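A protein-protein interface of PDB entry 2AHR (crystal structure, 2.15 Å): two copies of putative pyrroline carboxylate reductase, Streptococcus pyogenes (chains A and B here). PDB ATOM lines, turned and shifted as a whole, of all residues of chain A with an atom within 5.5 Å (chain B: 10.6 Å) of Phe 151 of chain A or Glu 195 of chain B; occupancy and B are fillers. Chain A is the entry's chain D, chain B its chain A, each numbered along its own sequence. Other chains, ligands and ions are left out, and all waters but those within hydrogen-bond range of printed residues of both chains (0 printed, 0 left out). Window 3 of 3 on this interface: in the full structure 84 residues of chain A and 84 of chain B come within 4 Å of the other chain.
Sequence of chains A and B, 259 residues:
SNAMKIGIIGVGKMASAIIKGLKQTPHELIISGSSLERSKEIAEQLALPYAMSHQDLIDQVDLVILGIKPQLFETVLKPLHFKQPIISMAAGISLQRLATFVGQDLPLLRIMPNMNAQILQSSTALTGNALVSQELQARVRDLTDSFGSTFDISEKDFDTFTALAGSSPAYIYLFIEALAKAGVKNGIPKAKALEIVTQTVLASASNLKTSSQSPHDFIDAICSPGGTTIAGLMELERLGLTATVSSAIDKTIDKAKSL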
ATOM      1  N   SER A 123      12.165  -9.226 -18.269  1.00  0.00           N
ATOM      2  CA  SER A 123      12.260  -9.163 -19.719  1.00  0.00           C
ATOM      3  C   SER A 123      10.834  -8.998 -20.237  1.00  0.00           C
ATOM      4  O   SER A 123      10.107  -9.990 -20.369  1.00  0.00           O
ATOM      5  CB  SER A 123      12.880 -10.446 -20.274  1.00  0.00           C
ATOM      6  OG  SER A 123      14.133 -10.687 -19.669  1.00  0.00           O
ATOM      7  N   THR A 124      10.458  -7.750 -20.533  1.00  0.00           N
ATOM      8  CA  THR A 124       9.063  -7.365 -20.753  1.00  0.00           C
ATOM      9  C   THR A 124       8.767  -6.963 -22.199  1.00  0.00           C
ATOM     10  O   THR A 124       9.371  -6.026 -22.723  1.00  0.00           O
ATOM     11  CB  THR A 124       8.656  -6.176 -19.863  1.00  0.00           C
ATOM     12  OG1 THR A 124       9.052  -6.404 -18.496  1.00  0.00           O
ATOM     13  CG2 THR A 124       7.158  -5.946 -19.936  1.00  0.00           C
ATOM     14  N   ALA A 125       7.822  -7.663 -22.817  1.00  0.00           N
ATOM     15  CA  ALA A 125       7.308  -7.307 -24.137  1.00  0.00           C
ATOM     16  C   ALA A 125       6.320  -6.163 -24.002  1.00  0.00           C
ATOM     17  O   ALA A 125       5.606  -6.067 -23.014  1.00  0.00           O
ATOM     18  CB  ALA A 125       6.608  -8.505 -24.769  1.00  0.00           C
ATOM     19  N   LEU A 126       6.253  -5.322 -25.023  1.00  0.00           N
ATOM     20  CA  LEU A 126       5.339  -4.188 -25.013  1.00  0.00           C
ATOM     21  C   LEU A 126       4.753  -4.011 -26.400  1.00  0.00           C
ATOM     22  O   LEU A 126       5.485  -4.058 -27.398  1.00  0.00           O
ATOM     23  CB  LEU A 126       6.080  -2.910 -24.604  1.00  0.00           C
ATOM     24  CG  LEU A 126       5.414  -1.544 -24.827  1.00  0.00           C
ATOM     25  CD1 LEU A 126       4.109  -1.412 -24.032  1.00  0.00           C
ATOM     26  CD2 LEU A 126       6.374  -0.404 -24.442  1.00  0.00           C
ATOM     27  N   ARG A 141       6.888   2.689 -22.197  1.00  0.00           N
ATOM     28  CA  ARG A 141       8.250   2.158 -22.246  1.00  0.00           C
ATOM     29  C   ARG A 141       9.061   2.576 -21.010  1.00  0.00           C
ATOM     30  O   ARG A 141       9.715   1.734 -20.399  1.00  0.00           O
ATOM     31  CB  ARG A 141       8.955   2.534 -23.552  1.00  0.00           C
ATOM     32  CG  ARG A 141      10.251   1.782 -23.832  1.00  0.00           C
ATOM     33  CD  ARG A 141      10.617   1.827 -25.318  1.00  0.00           C
ATOM     34  NE  ARG A 141       9.737   0.984 -26.143  1.00  0.00           N
ATOM     35  CZ  ARG A 141      10.079  -0.191 -26.682  1.00  0.00           C
ATOM     36  NH1 ARG A 141      11.299  -0.692 -26.509  1.00  0.00           N
ATOM     37  NH2 ARG A 141       9.192  -0.872 -27.411  1.00  0.00           N
ATOM     38  N   SER A 149      14.154  -4.659 -18.678  1.00  0.00           N
ATOM     39  CA  SER A 149      14.301  -4.227 -20.052  1.00  0.00           C
ATOM     40  C   SER A 149      12.955  -4.338 -20.749  1.00  0.00           C
ATOM     41  O   SER A 149      12.048  -5.008 -20.238  1.00  0.00           O
ATOM     42  CB  SER A 149      15.333  -5.073 -20.781  1.00  0.00           C
ATOM     43  OG  SER A 149      16.587  -5.027 -20.122  1.00  0.00           O
ATOM     44  N   THR A 150      12.833  -3.692 -21.911  1.00  0.00           N
ATOM     45  CA  THR A 150      11.600  -3.706 -22.691  1.00  0.00           C
ATOM     46  C   THR A 150      11.874  -4.131 -24.122  1.00  0.00           C
ATOM     47  O   THR A 150      12.817  -3.650 -24.754  1.00  0.00           O
ATOM     48  CB  THR A 150      10.901  -2.343 -22.668  1.00  0.00           C
ATOM     49  OG1 THR A 150      10.787  -1.897 -21.310  1.00  0.00           O
ATOM     50  CG2 THR A 150       9.513  -2.428 -23.274  1.00  0.00           C
ATOM     51  N   PHE A 151      11.056  -5.061 -24.612  1.00  0.00           N
ATOM     52  CA  PHE A 151      11.115  -5.508 -26.006  1.00  0.00           C
ATOM     53  C   PHE A 151       9.876  -5.049 -26.801  1.00  0.00           C
ATOM     54  O   PHE A 151       8.749  -5.350 -26.425  1.00  0.00           O
ATOM     55  CB  PHE A 151      11.259  -7.033 -26.082  1.00  0.00           C
ATOM     56  CG  PHE A 151      12.531  -7.563 -25.456  1.00  0.00           C
ATOM     57  CD1 PHE A 151      13.599  -7.966 -26.255  1.00  0.00           C
ATOM     58  CD2 PHE A 151      12.658  -7.663 -24.066  1.00  0.00           C
ATOM     59  CE1 PHE A 151      14.781  -8.454 -25.668  1.00  0.00           C
ATOM     60  CE2 PHE A 151      13.830  -8.162 -23.473  1.00  0.00           C
ATOM     61  CZ  PHE A 151      14.889  -8.552 -24.276  1.00  0.00           C
ATOM     62  N   ASP A 152      10.104  -4.320 -27.891  1.00  0.00           N
ATOM     63  CA  ASP A 152       9.037  -3.905 -28.792  1.00  0.00           C
ATOM     64  C   ASP A 152       8.752  -5.116 -29.647  1.00  0.00           C
ATOM     65  O   ASP A 152       9.483  -5.404 -30.593  1.00  0.00           O
ATOM     66  CB  ASP A 152       9.493  -2.713 -29.655  1.00  0.00           C
ATOM     67  CG  ASP A 152       8.588  -2.457 -30.876  1.00  0.00           C
ATOM     68  OD1 ASP A 152       7.389  -2.840 -30.874  1.00  0.00           O
ATOM     69  OD2 ASP A 152       9.087  -1.850 -31.855  1.00  0.00           O
ATOM     70  N   ILE A 153       7.719  -5.872 -29.303  1.00  0.00           N
ATOM     71  CA  ILE A 153       7.414  -7.034 -30.127  1.00  0.00           C
ATOM     72  C   ILE A 153       5.987  -6.973 -30.655  1.00  0.00           C
ATOM     73  O   ILE A 153       5.072  -6.458 -29.986  1.00  0.00           O
ATOM     74  CB  ILE A 153       7.705  -8.396 -29.430  1.00  0.00           C
ATOM     75  CG1 ILE A 153       6.554  -8.831 -28.552  1.00  0.00           C
ATOM     76  CG2 ILE A 153       9.056  -8.433 -28.656  1.00  0.00           C
ATOM     77  CD1 ILE A 153       6.337 -10.301 -28.690  1.00  0.00           C
ATOM     78  N   PHE A 161       6.379 -15.003 -26.842  1.00  0.00           N
ATOM     79  CA  PHE A 161       7.169 -14.236 -25.850  1.00  0.00           C
ATOM     80  C   PHE A 161       6.761 -14.647 -24.435  1.00  0.00           C
ATOM     81  O   PHE A 161       7.616 -14.824 -23.582  1.00  0.00           O
ATOM     82  CB  PHE A 161       7.029 -12.724 -26.044  1.00  0.00           C
ATOM     83  CG  PHE A 161       7.981 -11.911 -25.197  1.00  0.00           C
ATOM     84  CD1 PHE A 161       9.158 -11.395 -25.751  1.00  0.00           C
ATOM     85  CD2 PHE A 161       7.706 -11.664 -23.851  1.00  0.00           C
ATOM     86  CE1 PHE A 161      10.049 -10.638 -24.978  1.00  0.00           C
ATOM     87  CE2 PHE A 161       8.580 -10.921 -23.054  1.00  0.00           C
ATOM     88  CZ  PHE A 161       9.765 -10.395 -23.620  1.00  0.00           C
ATOM     89  N   ILE B 176      19.403 -23.509 -22.795  1.00  0.00           N
ATOM     90  CA  ILE B 176      19.167 -22.200 -23.374  1.00  0.00           C
ATOM     91  C   ILE B 176      18.885 -22.313 -24.872  1.00  0.00           C
ATOM     92  O   ILE B 176      17.929 -21.726 -25.384  1.00  0.00           O
ATOM     93  CB  ILE B 176      20.395 -21.275 -23.103  1.00  0.00           C
ATOM     94  CG1 ILE B 176      20.395 -20.811 -21.649  1.00  0.00           C
ATOM     95  CG2 ILE B 176      20.432 -20.079 -24.077  1.00  0.00           C
ATOM     96  CD1 ILE B 176      21.707 -20.190 -21.185  1.00  0.00           C
ATOM     97  N   GLU B 177      19.730 -23.057 -25.574  1.00  0.00           N
ATOM     98  CA  GLU B 177      19.569 -23.325 -27.001  1.00  0.00           C
ATOM     99  C   GLU B 177      18.214 -23.962 -27.307  1.00  0.00           C
ATOM    100  O   GLU B 177      17.600 -23.674 -28.346  1.00  0.00           O
ATOM    101  CB  GLU B 177      20.678 -24.285 -27.440  1.00  0.00           C
ATOM    102  CG  GLU B 177      20.659 -24.657 -28.921  1.00  0.00           C
ATOM    103  CD  GLU B 177      20.901 -23.464 -29.835  1.00  0.00           C
ATOM    104  OE1 GLU B 177      21.414 -22.416 -29.355  1.00  0.00           O
ATOM    105  OE2 GLU B 177      20.572 -23.577 -31.037  1.00  0.00           O
ATOM    106  N   LEU B 179      15.461 -23.540 -25.565  1.00  0.00           N
ATOM    107  CA  LEU B 179      14.451 -22.509 -25.375  1.00  0.00           C
ATOM    108  C   LEU B 179      14.385 -21.647 -26.627  1.00  0.00           C
ATOM    109  O   LEU B 179      13.304 -21.372 -27.141  1.00  0.00           O
ATOM    110  CB  LEU B 179      14.755 -21.645 -24.117  1.00  0.00           C
ATOM    111  CG  LEU B 179      14.497 -22.358 -22.765  1.00  0.00           C
ATOM    112  CD1 LEU B 179      14.957 -21.501 -21.585  1.00  0.00           C
ATOM    113  CD2 LEU B 179      13.000 -22.707 -22.617  1.00  0.00           C
ATOM    114  N   ALA B 180      15.550 -21.251 -27.125  1.00  0.00           N
ATOM    115  CA  ALA B 180      15.649 -20.375 -28.303  1.00  0.00           C
ATOM    116  C   ALA B 180      15.150 -21.033 -29.588  1.00  0.00           C
ATOM    117  O   ALA B 180      14.469 -20.392 -30.387  1.00  0.00           O
ATOM    118  CB  ALA B 180      17.082 -19.898 -28.473  1.00  0.00           C
ATOM    119  N   LYS B 181      15.508 -22.295 -29.798  1.00  0.00           N
ATOM    120  CA  LYS B 181      14.962 -23.101 -30.914  1.00  0.00           C
ATOM    121  C   LYS B 181      13.443 -23.203 -30.852  1.00  0.00           C
ATOM    122  O   LYS B 181      12.763 -23.161 -31.878  1.00  0.00           O
ATOM    123  CB  LYS B 181      15.575 -24.509 -30.915  1.00  0.00           C
ATOM    124  CG  LYS B 181      16.987 -24.616 -31.512  1.00  0.00           C
ATOM    125  CD  LYS B 181      16.957 -24.340 -32.996  1.00  0.00           C
ATOM    126  CE  LYS B 181      18.183 -24.863 -33.765  1.00  0.00           C
ATOM    127  NZ  LYS B 181      19.470 -24.799 -33.006  1.00  0.00           N
ATOM    128  N   GLY B 183      11.557 -20.942 -29.462  1.00  0.00           N
ATOM    129  CA  GLY B 183      11.243 -19.618 -30.008  1.00  0.00           C
ATOM    130  C   GLY B 183      11.216 -19.546 -31.526  1.00  0.00           C
ATOM    131  O   GLY B 183      10.261 -19.033 -32.090  1.00  0.00           O
ATOM    132  N   VAL B 184      12.253 -20.061 -32.192  1.00  0.00           N
ATOM    133  CA  VAL B 184      12.307 -20.084 -33.677  1.00  0.00           C
ATOM    134  C   VAL B 184      11.141 -20.868 -34.278  1.00  0.00           C
ATOM    135  O   VAL B 184      10.456 -20.388 -35.201  1.00  0.00           O
ATOM    136  CB  VAL B 184      13.657 -20.669 -34.197  1.00  0.00           C
ATOM    137  CG1 VAL B 184      13.654 -20.798 -35.738  1.00  0.00           C
ATOM    138  CG2 VAL B 184      14.793 -19.794 -33.764  1.00  0.00           C
ATOM    139  N   ILE B 188       9.795 -16.553 -33.671  1.00  0.00           N
ATOM    140  CA  ILE B 188      10.757 -15.519 -33.270  1.00  0.00           C
ATOM    141  C   ILE B 188      12.154 -15.858 -33.767  1.00  0.00           C
ATOM    142  O   ILE B 188      12.607 -16.988 -33.568  1.00  0.00           O
ATOM    143  CB  ILE B 188      10.731 -15.296 -31.748  1.00  0.00           C
ATOM    144  CG1 ILE B 188       9.336 -14.784 -31.325  1.00  0.00           C
ATOM    145  CG2 ILE B 188      11.854 -14.345 -31.321  1.00  0.00           C
ATOM    146  CD1 ILE B 188       9.176 -14.454 -29.836  1.00  0.00           C
ATOM    147  N   PRO B 189      12.840 -14.885 -34.424  1.00  0.00           N
ATOM    148  CA  PRO B 189      14.200 -15.072 -34.963  1.00  0.00           C
ATOM    149  C   PRO B 189      15.175 -15.574 -33.899  1.00  0.00           C
ATOM    150  O   PRO B 189      15.101 -15.135 -32.750  1.00  0.00           O
ATOM    151  CB  PRO B 189      14.628 -13.644 -35.364  1.00  0.00           C
ATOM    152  CG  PRO B 189      13.364 -12.897 -35.581  1.00  0.00           C
ATOM    153  CD  PRO B 189      12.338 -13.513 -34.658  1.00  0.00           C
ATOM    154  N   LYS B 190      16.106 -16.439 -34.299  1.00  0.00           N
ATOM    155  CA  LYS B 190      17.055 -17.089 -33.369  1.00  0.00           C
ATOM    156  C   LYS B 190      17.809 -16.130 -32.453  1.00  0.00           C
ATOM    157  O   LYS B 190      17.887 -16.382 -31.250  1.00  0.00           O
ATOM    158  CB  LYS B 190      18.057 -17.990 -34.127  1.00  0.00           C
ATOM    159  CG  LYS B 190      19.102 -18.714 -33.205  1.00  0.00           C
ATOM    160  CD  LYS B 190      18.458 -19.958 -32.506  1.00  0.00           C
ATOM    161  CE  LYS B 190      19.366 -20.604 -31.477  1.00  0.00           C
ATOM    162  NZ  LYS B 190      20.709 -21.048 -31.996  1.00  0.00           N
ATOM    163  N   ALA B 191      18.367 -15.048 -33.025  1.00  0.00           N
ATOM    164  CA  ALA B 191      19.143 -14.064 -32.259  1.00  0.00           C
ATOM    165  C   ALA B 191      18.303 -13.368 -31.200  1.00  0.00           C
ATOM    166  O   ALA B 191      18.766 -13.150 -30.081  1.00  0.00           O
ATOM    167  CB  ALA B 191      19.790 -13.001 -33.197  1.00  0.00           C
ATOM    168  N   LYS B 192      17.076 -13.012 -31.565  1.00  0.00           N
ATOM    169  CA  LYS B 192      16.162 -12.329 -30.667  1.00  0.00           C
ATOM    170  C   LYS B 192      15.708 -13.254 -29.539  1.00  0.00           C
ATOM    171  O   LYS B 192      15.671 -12.843 -28.387  1.00  0.00           O
ATOM    172  CB  LYS B 192      14.955 -11.817 -31.458  1.00  0.00           C
ATOM    173  CG  LYS B 192      13.919 -11.024 -30.664  1.00  0.00           C
ATOM    174  CD  LYS B 192      14.523  -9.896 -29.836  1.00  0.00           C
ATOM    175  CE  LYS B 192      15.179  -8.826 -30.710  1.00  0.00           C
ATOM    176  NZ  LYS B 192      15.794  -7.750 -29.883  1.00  0.00           N
ATOM    177  N   ALA B 193      15.380 -14.501 -29.875  1.00  0.00           N
ATOM    178  CA  ALA B 193      14.943 -15.474 -28.866  1.00  0.00           C
ATOM    179  C   ALA B 193      16.061 -15.757 -27.877  1.00  0.00           C
ATOM    180  O   ALA B 193      15.827 -15.866 -26.680  1.00  0.00           O
ATOM    181  CB  ALA B 193      14.471 -16.771 -29.539  1.00  0.00           C
ATOM    182  N   LEU B 194      17.284 -15.837 -28.392  1.00  0.00           N
ATOM    183  CA  LEU B 194      18.454 -16.096 -27.588  1.00  0.00           C
ATOM    184  C   LEU B 194      18.757 -14.911 -26.651  1.00  0.00           C
ATOM    185  O   LEU B 194      19.140 -15.113 -25.490  1.00  0.00           O
ATOM    186  CB  LEU B 194      19.629 -16.369 -28.528  1.00  0.00           C
ATOM    187  CG  LEU B 194      20.797 -17.283 -28.191  1.00  0.00           C
ATOM    188  CD1 LEU B 194      20.373 -18.607 -27.506  1.00  0.00           C
ATOM    189  CD2 LEU B 194      21.529 -17.569 -29.524  1.00  0.00           C
ATOM    190  N   GLU B 195      18.580 -13.685 -27.161  1.00  0.00           N
ATOM    191  CA  GLU B 195      18.705 -12.482 -26.342  1.00  0.00           C
ATOM    192  C   GLU B 195      17.662 -12.536 -25.206  1.00  0.00           C
ATOM    193  O   GLU B 195      18.010 -12.407 -24.033  1.00  0.00           O
ATOM    194  CB  GLU B 195      18.541 -11.223 -27.198  1.00  0.00           C
ATOM    195  CG  GLU B 195      18.646  -9.903 -26.407  1.00  0.00           C
ATOM    196  CD  GLU B 195      18.272  -8.656 -27.228  1.00  0.00           C
ATOM    197  OE1 GLU B 195      17.924  -8.786 -28.427  1.00  0.00           O
ATOM    198  OE2 GLU B 195      18.317  -7.531 -26.659  1.00  0.00           O
ATOM    199  N   ILE B 196      16.395 -12.769 -25.550  1.00  0.00           N
ATOM    200  CA  ILE B 196      15.334 -12.843 -24.532  1.00  0.00           C
ATOM    201  C   ILE B 196      15.669 -13.896 -23.456  1.00  0.00           C
ATOM    202  O   ILE B 196      15.703 -13.586 -22.258  1.00  0.00           O
ATOM    203  CB  ILE B 196      13.947 -13.144 -25.165  1.00  0.00           C
ATOM    204  CG1 ILE B 196      13.485 -11.963 -26.025  1.00  0.00           C
ATOM    205  CG2 ILE B 196      12.889 -13.467 -24.085  1.00  0.00           C
ATOM    206  CD1 ILE B 196      12.459 -12.340 -27.075  1.00  0.00           C
ATOM    207  N   VAL B 197      15.971 -15.114 -23.913  1.00  0.00           N
ATOM    208  CA  VAL B 197      16.154 -16.256 -23.025  1.00  0.00           C
ATOM    209  C   VAL B 197      17.389 -16.109 -22.132  1.00  0.00           C
ATOM    210  O   VAL B 197      17.318 -16.362 -20.922  1.00  0.00           O
ATOM    211  CB  VAL B 197      16.196 -17.606 -23.820  1.00  0.00           C
ATOM    212  CG1 VAL B 197      16.750 -18.721 -22.953  1.00  0.00           C
ATOM    213  CG2 VAL B 197      14.805 -17.947 -24.301  1.00  0.00           C
ATOM    214  N   THR B 198      18.513 -15.722 -22.740  1.00  0.00           N
ATOM    215  CA  THR B 198      19.756 -15.526 -22.013  1.00  0.00           C
ATOM    216  C   THR B 198      19.567 -14.498 -20.885  1.00  0.00           C
ATOM    217  O   THR B 198      20.005 -14.693 -19.746  1.00  0.00           O
ATOM    218  CB  THR B 198      20.896 -15.052 -22.991  1.00  0.00           C
ATOM    219  OG1 THR B 198      21.116 -16.062 -23.978  1.00  0.00           O
ATOM    220  CG2 THR B 198      22.196 -14.808 -22.269  1.00  0.00           C
ATOM    221  N   GLN B 199      18.920 -13.388 -21.228  1.00  0.00           N
ATOM    222  CA  GLN B 199      18.648 -12.322 -20.270  1.00  0.00           C
ATOM    223  C   GLN B 199      17.692 -12.836 -19.180  1.00  0.00           C
ATOM    224  O   GLN B 199      17.845 -12.503 -18.001  1.00  0.00           O
ATOM    225  CB  GLN B 199      18.038 -11.142 -21.020  1.00  0.00           C
ATOM    226  CG  GLN B 199      17.811  -9.884 -20.186  1.00  0.00           C
ATOM    227  CD  GLN B 199      17.102  -8.775 -20.992  1.00  0.00           C
ATOM    228  OE1 GLN B 199      17.674  -8.229 -21.964  1.00  0.00           O
ATOM    229  NE2 GLN B 199      15.855  -8.450 -20.594  1.00  0.00           N
ATOM    230  N   THR B 200      16.715 -13.659 -19.564  1.00  0.00           N
ATOM    231  CA  THR B 200      15.802 -14.219 -18.574  1.00  0.00           C
ATOM    232  C   THR B 200      16.541 -15.201 -17.636  1.00  0.00           C
ATOM    233  O   THR B 200      16.301 -15.187 -16.418  1.00  0.00           O
ATOM    234  CB  THR B 200      14.542 -14.855 -19.226  1.00  0.00           C
ATOM    235  OG1 THR B 200      13.815 -13.838 -19.925  1.00  0.00           O
ATOM    236  CG2 THR B 200      13.606 -15.458 -18.179  1.00  0.00           C
ATOM    237  N   VAL B 201      17.425 -16.038 -18.187  1.00  0.00           N
ATOM    238  CA  VAL B 201      18.188 -17.017 -17.366  1.00  0.00           C
ATOM    239  C   VAL B 201      19.092 -16.252 -16.387  1.00  0.00           C
ATOM    240  O   VAL B 201      19.136 -16.514 -15.173  1.00  0.00           O
ATOM    241  CB  VAL B 201      19.062 -17.946 -18.229  1.00  0.00           C
ATOM    242  CG1 VAL B 201      20.064 -18.716 -17.348  1.00  0.00           C
ATOM    243  CG2 VAL B 201      18.195 -18.936 -19.015  1.00  0.00           C
ATOM    244  N   LEU B 202      19.819 -15.296 -16.938  1.00  0.00           N
ATOM    245  CA  LEU B 202      20.663 -14.444 -16.131  1.00  0.00           C
ATOM    246  C   LEU B 202      19.903 -13.840 -14.955  1.00  0.00           C
ATOM    247  O   LEU B 202      20.346 -13.971 -13.818  1.00  0.00           O
ATOM    248  CB  LEU B 202      21.291 -13.368 -17.021  1.00  0.00           C
ATOM    249  CG  LEU B 202      22.396 -12.505 -16.453  1.00  0.00           C
ATOM    250  CD1 LEU B 202      23.528 -13.353 -15.908  1.00  0.00           C
ATOM    251  CD2 LEU B 202      22.903 -11.611 -17.572  1.00  0.00           C
ATOM    252  N   ALA B 203      18.756 -13.205 -15.213  1.00  0.00           N
ATOM    253  CA  ALA B 203      17.975 -12.531 -14.160  1.00  0.00           C
ATOM    254  C   ALA B 203      17.382 -13.507 -13.151  1.00  0.00           C
ATOM    255  O   ALA B 203      17.352 -13.231 -11.939  1.00  0.00           O
ATOM    256  CB  ALA B 203      16.855 -11.680 -14.779  1.00  0.00           C
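The side-chain hydroxyl of Thr 200 of chain B sits at hydrogen-bond distance from the side-chain hydroxyl of Ser 123 of chain A, at 3.2 Å. The side-chain amide nitrogen (NE2) of Gln 199 of chain B is in hydrogen-bond range of the side-chain hydroxyl (OG) of Ser 123 of chain A (3.0 Å).
The side-chain carboxylate (OE1) of Glu 195 of chain B lies within salt-bridge range of the side-chain amino group (NZ) of Lys 192 of chain B. The backbone carbonyl oxygen (O) of Thr 124 of chain A is in hydrogen-bond range of the backbone NH (N) of Phe 151 of chain A (2.7 Å). O of Ile 196 of chain B lies within hydrogen-bond range of OG1 of Thr 200 of chain B, at 3.0 Å. O of Phe 151 of chain A is in hydrogen-bond range of N of Leu 126 of chain A (2.9 Å). The backbone NH (N) of Thr 124 of chain A lies within hydrogen-bond range of the backbone carbonyl oxygen (O) of Ser 149 of chain A (3.2 Å).
CB of Ser 149 of chain A touches NE2 of Gln 199 of chain B (3.4 Å). Glu 195 of chain B touches Phe 151 of chain A. Ile 196 of chain B touches Phe 151 of chain A. CE2 of Phe 151 of chain A touches NE2 of Gln 199 of chain B, at 3.5 Å. CE1 of Phe 161 of chain A touches CD1 of Ile 196 of chain B, at 3.6 Å.
Ser 123 of chain A touches just these residues of chain B: Gln 199 (3.0 Å) and Thr 200 (3.2 Å). No residue of chain B comes within 4 Å of Ala 125 of chain A. Thr 150 of chain A touches none of the printed residues of chain B. No residue of chain B comes within 4 Å of Asp 152 of chain A. No residue of chain B comes within 4 Å of Ile 153 of chain A. Printed residues of chain B within 4 Å of Phe 161 of chain A: Ile 196 (3.6 Å). Gly 183 of chain B touches none of the printed residues of chain A. Glu 195 of chain B touches just one residue of chain A: Phe 151 (3.8 Å). Val 197 of chain B touches none of the printed residues of chain A. Of the printed residues of chain A, Thr 200 of chain B touches Ser 123 (3.2 Å). The nearest printed residue of chain A that does not touch Thr 200 of chain B is Phe 161 of chain A (6.5 Å).
Printed residues of chain B that touch a printed residue of chain A: Glu 195, Ile 196, Gln 199 and Thr 200. Hydrophobic or aromatic side chains of chain B within 4 Å of the printed part of chain A: Ile 196. Along chain B the printed residues that touch a printed residue of chain A span positions 195 to 200. Printed residues of chain A that touch a printed residue of chain B: Ser 123, Ser 149, Phe 151 and Phe 161. Among the printed residues, no Asp or Glu carboxylate lies within 4 Å of a Lys or Arg side-chain nitrogen of the other chain.
No position is printed for both chains. Of the 7 pairs that touch across the chains among the printed residues, none has its exchanged pair printed and touching as well.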
